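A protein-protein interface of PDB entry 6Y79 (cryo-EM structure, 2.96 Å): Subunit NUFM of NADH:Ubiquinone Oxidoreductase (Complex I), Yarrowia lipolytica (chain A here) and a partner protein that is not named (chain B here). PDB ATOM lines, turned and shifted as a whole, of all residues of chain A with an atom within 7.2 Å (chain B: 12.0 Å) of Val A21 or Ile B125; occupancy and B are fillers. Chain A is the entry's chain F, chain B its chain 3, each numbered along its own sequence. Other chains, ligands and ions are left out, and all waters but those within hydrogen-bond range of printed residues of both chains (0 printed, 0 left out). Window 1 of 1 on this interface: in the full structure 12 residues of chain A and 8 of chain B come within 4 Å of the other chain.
OG of Ser B123 is in hydrogen-bond range of O of Gln A24 (2.9 Å).
The backbone carbonyl oxygen (O) of Leu B124 lies within hydrogen-bond range of the backbone NH (N) of Val A23.
The backbone NH (N) of Leu B124 sits at hydrogen-bond distance from the backbone carbonyl oxygen (O) of Gln A24 (3.1 Å).
The backbone carbonyl oxygen of Val A21 sits at hydrogen-bond distance from the backbone NH of Tyr B126.
The backbone carbonyl oxygen of Gln A19 sits close to the backbone carbonyl oxygen of Lys B127 (2.9 Å).
Of the 15 printed residues of chain A, 8 touch a printed residue of chain B.
Printed residues of chain A that touch a printed residue of chain B: Gln A19, Ser A20, Val A21, Leu A22, Val A23, Gln A24, His A108 and Leu A111.
Hydrophobic or aromatic side chains of chain A that line the printed part of chain B: Val A21, Leu A22, Val A23, His A108 and Leu A111.
Hydrophobic or aromatic side chains of chain B within 4 Å of the printed part of chain A: Leu B124, Ile B125 and Tyr B126.
Among the printed residues, 12 pairs touch across the chains.
Among the printed residues, no Asp or Glu carboxylate lies within 4 Å of a Lys or Arg side-chain nitrogen of the other chain.
Ser A20 touches Tyr B126 (CA to O, 3.2 Å).
CB of Ser A20 touches O of Lys B127 (3.4 Å).
O of Val A21 touches CA of Ile B125 (3.3 Å).
CD2 of Leu A22 touches OG of Ser B123 (3.6 Å).
Leu B124 touches Leu A22 (O to CA, 3.7 Å).
CE1 of His A108 touches CD1 of Tyr B126, at 3.3 Å.
Leu A111 touches Tyr B126 (CD2 to CE2, 3.6 Å).
Val A21 touches just these residues of chain B: Ile B125 (3.3 Å) and Tyr B126 (2.9 Å).
Ile B125 touches one residue of chain A.
Gln A19 touches one residue of chain B.
Of chain B, only Tyr B126 (3.2 Å) and Lys B127 (3.4 Å) come within 4 Å of Ser A20.
Leu A22 touches just these residues of chain B: Ser B123 and Leu B124.
Val A23 touches one residue of chain B.
No residue of chain B comes within 4 Å of Ala A45.
No residue of chain B comes within 4 Å of Ala A48.
Leu A49 touches none of the printed residues of chain B.
Of the printed residues of chain B, Gln A24 touches Ser B123 and Leu B124.
Of the printed residues of chain A, Ser B123 touches Leu A22 (3.6 Å) and Gln A24 (2.9 Å).
Of the printed residues of chain B, Leu A111 touches Tyr B126.
Of the printed residues of chain A, Lys B127 touches Gln A19 (2.9 Å) and Ser A20 (3.4 Å).
Printed residues of chain A within 4 Å of Tyr B126: Ser A20, Val A21, His A108 and Leu A111.
Leu A46 touches none of the printed residues of chain B.
The nearest residue of chain B that does not touch Val A21 is Leu B124 (4.2 Å).
The nearest residue of chain A that does not touch Ile B125 is Leu A22 (4.4 Å).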
ATOM      1  N   GLN A  19     -27.402 -20.073  13.303  1.00  0.00           N
ATOM      2  CA  GLN A  19     -27.866 -20.985  12.264  1.00  0.00           C
ATOM      3  C   GLN A  19     -27.311 -20.598  10.901  1.00  0.00           C
ATOM      4  O   GLN A  19     -26.817 -19.488  10.718  1.00  0.00           O
ATOM      5  CB  GLN A  19     -29.389 -21.004  12.213  1.00  0.00           C
ATOM      6  CG  GLN A  19     -29.990 -19.684  11.792  1.00  0.00           C
ATOM      7  CD  GLN A  19     -31.493 -19.734  11.731  1.00  0.00           C
ATOM      8  OE1 GLN A  19     -32.099 -20.781  11.957  1.00  0.00           O
ATOM      9  NE2 GLN A  19     -32.111 -18.603  11.415  1.00  0.00           N
ATOM     10  N   SER A  20     -27.406 -21.515   9.942  1.00  0.00           N
ATOM     11  CA  SER A  20     -26.858 -21.290   8.614  1.00  0.00           C
ATOM     12  C   SER A  20     -27.868 -21.711   7.559  1.00  0.00           C
ATOM     13  O   SER A  20     -28.635 -22.658   7.751  1.00  0.00           O
ATOM     14  CB  SER A  20     -25.538 -22.042   8.409  1.00  0.00           C
ATOM     15  OG  SER A  20     -25.740 -23.441   8.404  1.00  0.00           O
ATOM     16  N   VAL A  21     -27.848 -21.006   6.432  1.00  0.00           N
ATOM     17  CA  VAL A  21     -28.877 -21.134   5.409  1.00  0.00           C
ATOM     18  C   VAL A  21     -28.215 -21.402   4.062  1.00  0.00           C
ATOM     19  O   VAL A  21     -27.101 -20.937   3.793  1.00  0.00           O
ATOM     20  CB  VAL A  21     -29.778 -19.866   5.392  1.00  0.00           C
ATOM     21  CG1 VAL A  21     -29.033 -18.625   4.903  1.00  0.00           C
ATOM     22  CG2 VAL A  21     -31.046 -20.094   4.610  1.00  0.00           C
ATOM     23  N   LEU A  22     -28.875 -22.209   3.229  1.00  0.00           N
ATOM     24  CA  LEU A  22     -28.389 -22.472   1.882  1.00  0.00           C
ATOM     25  C   LEU A  22     -29.053 -21.513   0.908  1.00  0.00           C
ATOM     26  O   LEU A  22     -30.263 -21.271   0.975  1.00  0.00           O
ATOM     27  CB  LEU A  22     -28.651 -23.915   1.441  1.00  0.00           C
ATOM     28  CG  LEU A  22     -27.766 -24.490   0.325  1.00  0.00           C
ATOM     29  CD1 LEU A  22     -27.636 -25.976   0.562  1.00  0.00           C
ATOM     30  CD2 LEU A  22     -28.240 -24.233  -1.113  1.00  0.00           C
ATOM     31  N   VAL A  23     -28.245 -20.985  -0.006  1.00  0.00           N
ATOM     32  CA  VAL A  23     -28.709 -20.066  -1.033  1.00  0.00           C
ATOM     33  C   VAL A  23     -28.618 -20.651  -2.436  1.00  0.00           C
ATOM     34  O   VAL A  23     -29.574 -20.512  -3.219  1.00  0.00           O
ATOM     35  CB  VAL A  23     -27.927 -18.738  -0.965  1.00  0.00           C
ATOM     36  CG1 VAL A  23     -28.453 -17.767  -1.986  1.00  0.00           C
ATOM     37  CG2 VAL A  23     -28.010 -18.147   0.427  1.00  0.00           C
ATOM     38  N   GLN A  24     -27.529 -21.325  -2.798  1.00  0.00           N
ATOM     39  CA  GLN A  24     -27.367 -21.795  -4.168  1.00  0.00           C
ATOM     40  C   GLN A  24     -26.739 -23.177  -4.167  1.00  0.00           C
ATOM     41  O   GLN A  24     -25.607 -23.342  -3.707  1.00  0.00           O
ATOM     42  CB  GLN A  24     -26.511 -20.830  -4.980  1.00  0.00           C
ATOM     43  CG  GLN A  24     -26.323 -21.246  -6.420  1.00  0.00           C
ATOM     44  CD  GLN A  24     -25.503 -20.249  -7.192  1.00  0.00           C
ATOM     45  OE1 GLN A  24     -25.150 -19.192  -6.677  1.00  0.00           O
ATOM     46  NE2 GLN A  24     -25.174 -20.585  -8.430  1.00  0.00           N
ATOM     47  N   HIS A  39     -32.847 -26.526  -5.960  1.00  0.00           N
ATOM     48  CA  HIS A  39     -32.543 -26.166  -4.594  1.00  0.00           C
ATOM     49  C   HIS A  39     -33.587 -26.767  -3.673  1.00  0.00           C
ATOM     50  O   HIS A  39     -34.769 -26.404  -3.776  1.00  0.00           O
ATOM     51  CB  HIS A  39     -32.508 -24.648  -4.477  1.00  0.00           C
ATOM     52  CG  HIS A  39     -32.545 -24.124  -3.080  1.00  0.00           C
ATOM     53  ND1 HIS A  39     -31.464 -24.168  -2.225  1.00  0.00           N
ATOM     54  CD2 HIS A  39     -33.524 -23.480  -2.415  1.00  0.00           C
ATOM     55  CE1 HIS A  39     -31.794 -23.607  -1.076  1.00  0.00           C
ATOM     56  NE2 HIS A  39     -33.041 -23.186  -1.165  1.00  0.00           N
ATOM     57  N   PRO A  44     -38.619 -21.921   3.103  1.00  0.00           N
ATOM     58  CA  PRO A  44     -37.937 -21.600   4.379  1.00  0.00           C
ATOM     59  C   PRO A  44     -36.629 -20.821   4.278  1.00  0.00           C
ATOM     60  O   PRO A  44     -36.433 -19.887   5.073  1.00  0.00           O
ATOM     61  CB  PRO A  44     -37.733 -22.978   5.005  1.00  0.00           C
ATOM     62  CG  PRO A  44     -38.992 -23.654   4.648  1.00  0.00           C
ATOM     63  CD  PRO A  44     -39.285 -23.214   3.232  1.00  0.00           C
ATOM     64  N   ALA A  45     -35.729 -21.179   3.358  1.00  0.00           N
ATOM     65  CA  ALA A  45     -34.522 -20.384   3.139  1.00  0.00           C
ATOM     66  C   ALA A  45     -34.874 -18.979   2.677  1.00  0.00           C
ATOM     67  O   ALA A  45     -34.278 -17.995   3.135  1.00  0.00           O
ATOM     68  CB  ALA A  45     -33.617 -21.067   2.115  1.00  0.00           C
ATOM     69  N   LEU A  46     -35.894 -18.877   1.823  1.00  0.00           N
ATOM     70  CA  LEU A  46     -36.381 -17.599   1.320  1.00  0.00           C
ATOM     71  C   LEU A  46     -36.928 -16.724   2.443  1.00  0.00           C
ATOM     72  O   LEU A  46     -36.571 -15.545   2.560  1.00  0.00           O
ATOM     73  CB  LEU A  46     -37.463 -17.876   0.278  1.00  0.00           C
ATOM     74  CG  LEU A  46     -37.885 -16.853  -0.760  1.00  0.00           C
ATOM     75  CD1 LEU A  46     -36.664 -16.206  -1.358  1.00  0.00           C
ATOM     76  CD2 LEU A  46     -38.671 -17.570  -1.829  1.00  0.00           C
ATOM     77  N   ALA A  48     -36.442 -17.034   5.745  1.00  0.00           N
ATOM     78  CA  ALA A  48     -35.419 -16.710   6.735  1.00  0.00           C
ATOM     79  C   ALA A  48     -34.483 -15.619   6.232  1.00  0.00           C
ATOM     80  O   ALA A  48     -34.082 -14.735   7.004  1.00  0.00           O
ATOM     81  CB  ALA A  48     -34.633 -17.970   7.095  1.00  0.00           C
ATOM     82  N   LEU A  49     -34.165 -15.644   4.933  1.00  0.00           N
ATOM     83  CA  LEU A  49     -33.383 -14.582   4.308  1.00  0.00           C
ATOM     84  C   LEU A  49     -34.121 -13.246   4.355  1.00  0.00           C
ATOM     85  O   LEU A  49     -33.521 -12.205   4.657  1.00  0.00           O
ATOM     86  CB  LEU A  49     -33.083 -14.992   2.870  1.00  0.00           C
ATOM     87  CG  LEU A  49     -31.778 -14.719   2.134  1.00  0.00           C
ATOM     88  CD1 LEU A  49     -30.568 -14.904   3.014  1.00  0.00           C
ATOM     89  CD2 LEU A  49     -31.712 -15.697   0.973  1.00  0.00           C
ATOM     90  N   VAL A 104     -33.743 -16.699  -4.536  1.00  0.00           N
ATOM     91  CA  VAL A 104     -33.017 -16.881  -3.286  1.00  0.00           C
ATOM     92  C   VAL A 104     -31.622 -16.265  -3.385  1.00  0.00           C
ATOM     93  O   VAL A 104     -31.139 -15.639  -2.425  1.00  0.00           O
ATOM     94  CB  VAL A 104     -32.989 -18.377  -2.908  1.00  0.00           C
ATOM     95  CG1 VAL A 104     -32.098 -18.628  -1.714  1.00  0.00           C
ATOM     96  CG2 VAL A 104     -34.390 -18.861  -2.563  1.00  0.00           C
ATOM     97  N   HIS A 108     -30.403 -13.128  -0.938  1.00  0.00           N
ATOM     98  CA  HIS A 108     -29.086 -13.137  -0.313  1.00  0.00           C
ATOM     99  C   HIS A 108     -28.271 -11.917  -0.711  1.00  0.00           C
ATOM    100  O   HIS A 108     -27.542 -11.337   0.113  1.00  0.00           O
ATOM    101  CB  HIS A 108     -28.370 -14.403  -0.727  1.00  0.00           C
ATOM    102  CG  HIS A 108     -26.965 -14.503  -0.245  1.00  0.00           C
ATOM    103  ND1 HIS A 108     -26.650 -14.902   1.032  1.00  0.00           N
ATOM    104  CD2 HIS A 108     -25.789 -14.295  -0.879  1.00  0.00           C
ATOM    105  CE1 HIS A 108     -25.338 -14.921   1.170  1.00  0.00           C
ATOM    106  NE2 HIS A 108     -24.791 -14.556   0.025  1.00  0.00           N
ATOM    107  N   LEU A 111     -29.475  -8.863   0.984  1.00  0.00           N
ATOM    108  CA  LEU A 111     -29.103  -8.926   2.394  1.00  0.00           C
ATOM    109  C   LEU A 111     -27.673  -8.445   2.615  1.00  0.00           C
ATOM    110  O   LEU A 111     -27.412  -7.640   3.520  1.00  0.00           O
ATOM    111  CB  LEU A 111     -29.278 -10.348   2.925  1.00  0.00           C
ATOM    112  CG  LEU A 111     -28.751 -10.591   4.344  1.00  0.00           C
ATOM    113  CD1 LEU A 111     -29.463  -9.722   5.368  1.00  0.00           C
ATOM    114  CD2 LEU A 111     -28.897 -12.035   4.709  1.00  0.00           C
ATOM    115  N   ASN B 120     -15.789 -26.791  -8.806  1.00  0.00           N
ATOM    116  CA  ASN B 120     -15.900 -26.548  -7.358  1.00  0.00           C
ATOM    117  C   ASN B 120     -17.352 -26.701  -6.890  1.00  0.00           C
ATOM    118  O   ASN B 120     -18.062 -25.744  -6.598  1.00  0.00           O
ATOM    119  CB  ASN B 120     -15.300 -25.204  -6.922  1.00  0.00           C
ATOM    120  CG  ASN B 120     -14.987 -25.153  -5.407  1.00  0.00           C
ATOM    121  OD1 ASN B 120     -15.346 -26.063  -4.657  1.00  0.00           O
ATOM    122  ND2 ASN B 120     -14.267 -24.123  -4.977  1.00  0.00           N
ATOM    123  N   THR B 121     -17.785 -27.951  -6.877  1.00  0.00           N
ATOM    124  CA  THR B 121     -19.096 -28.444  -6.463  1.00  0.00           C
ATOM    125  C   THR B 121     -19.628 -27.932  -5.115  1.00  0.00           C
ATOM    126  O   THR B 121     -20.840 -28.011  -4.896  1.00  0.00           O
ATOM    127  CB  THR B 121     -18.958 -29.955  -6.416  1.00  0.00           C
ATOM    128  OG1 THR B 121     -18.118 -30.287  -5.303  1.00  0.00           O
ATOM    129  CG2 THR B 121     -18.275 -30.413  -7.660  1.00  0.00           C
ATOM    130  N   ASP B 122     -18.790 -27.430  -4.206  1.00  0.00           N
ATOM    131  CA  ASP B 122     -19.232 -27.207  -2.831  1.00  0.00           C
ATOM    132  C   ASP B 122     -20.129 -25.973  -2.712  1.00  0.00           C
ATOM    133  O   ASP B 122     -19.771 -24.882  -3.165  1.00  0.00           O
ATOM    134  CB  ASP B 122     -18.025 -27.093  -1.903  1.00  0.00           C
ATOM    135  CG  ASP B 122     -17.403 -28.449  -1.588  1.00  0.00           C
ATOM    136  OD1 ASP B 122     -17.693 -29.430  -2.305  1.00  0.00           O
ATOM    137  OD2 ASP B 122     -16.623 -28.533  -0.619  1.00  0.00           O
ATOM    138  N   SER B 123     -21.272 -26.150  -2.044  1.00  0.00           N
ATOM    139  CA  SER B 123     -22.444 -25.294  -2.175  1.00  0.00           C
ATOM    140  C   SER B 123     -22.259 -23.939  -1.489  1.00  0.00           C
ATOM    141  O   SER B 123     -21.251 -23.663  -0.833  1.00  0.00           O
ATOM    142  CB  SER B 123     -23.671 -25.992  -1.597  1.00  0.00           C
ATOM    143  OG  SER B 123     -24.801 -25.141  -1.627  1.00  0.00           O
ATOM    144  N   LEU B 124     -23.276 -23.088  -1.651  1.00  0.00           N
ATOM    145  CA  LEU B 124     -23.265 -21.708  -1.163  1.00  0.00           C
ATOM    146  C   LEU B 124     -24.112 -21.626   0.103  1.00  0.00           C
ATOM    147  O   LEU B 124     -25.341 -21.521   0.043  1.00  0.00           O
ATOM    148  CB  LEU B 124     -23.776 -20.752  -2.237  1.00  0.00           C
ATOM    149  CG  LEU B 124     -23.828 -19.262  -1.884  1.00  0.00           C
ATOM    150  CD1 LEU B 124     -22.473 -18.785  -1.396  1.00  0.00           C
ATOM    151  CD2 LEU B 124     -24.299 -18.435  -3.065  1.00  0.00           C
ATOM    152  N   ILE B 125     -23.442 -21.659   1.248  1.00  0.00           N
ATOM    153  CA  ILE B 125     -24.087 -21.561   2.545  1.00  0.00           C
ATOM    154  C   ILE B 125     -23.803 -20.174   3.111  1.00  0.00           C
ATOM    155  O   ILE B 125     -22.975 -19.427   2.593  1.00  0.00           O
ATOM    156  CB  ILE B 125     -23.611 -22.666   3.503  1.00  0.00           C
ATOM    157  CG1 ILE B 125     -22.098 -22.562   3.687  1.00  0.00           C
ATOM    158  CG2 ILE B 125     -23.979 -24.030   2.952  1.00  0.00           C
ATOM    159  CD1 ILE B 125     -21.521 -23.574   4.635  1.00  0.00           C
ATOM    160  N   TYR B 126     -24.493 -19.832   4.194  1.00  0.00           N
ATOM    161  CA  TYR B 126     -24.377 -18.466   4.684  1.00  0.00           C
ATOM    162  C   TYR B 126     -24.493 -18.411   6.201  1.00  0.00           C
ATOM    163  O   TYR B 126     -25.272 -19.156   6.789  1.00  0.00           O
ATOM    164  CB  TYR B 126     -25.440 -17.568   4.049  1.00  0.00           C
ATOM    165  CG  TYR B 126     -25.245 -16.130   4.422  1.00  0.00           C
ATOM    166  CD1 TYR B 126     -24.024 -15.502   4.193  1.00  0.00           C
ATOM    167  CD2 TYR B 126     -26.254 -15.409   5.037  1.00  0.00           C
ATOM    168  CE1 TYR B 126     -23.828 -14.186   4.538  1.00  0.00           C
ATOM    169  CE2 TYR B 126     -26.063 -14.093   5.395  1.00  0.00           C
ATOM    170  CZ  TYR B 126     -24.851 -13.488   5.139  1.00  0.00           C
ATOM    171  OH  TYR B 126     -24.659 -12.175   5.490  1.00  0.00           O
ATOM    172  N   LYS B 127     -23.695 -17.525   6.808  1.00  0.00           N
ATOM    173  CA  LYS B 127     -23.766 -17.099   8.214  1.00  0.00           C
ATOM    174  C   LYS B 127     -23.444 -18.215   9.205  1.00  0.00           C
ATOM    175  O   LYS B 127     -24.246 -19.111   9.451  1.00  0.00           O
ATOM    176  CB  LYS B 127     -25.140 -16.488   8.521  1.00  0.00           C
ATOM    177  CG  LYS B 127     -25.301 -15.955   9.928  1.00  0.00           C
ATOM    178  CD  LYS B 127     -26.637 -15.253  10.085  1.00  0.00           C
ATOM    179  CE  LYS B 127     -27.784 -16.254  10.090  1.00  0.00           C
ATOM    180  NZ  LYS B 127     -29.098 -15.605  10.373  1.00  0.00           N
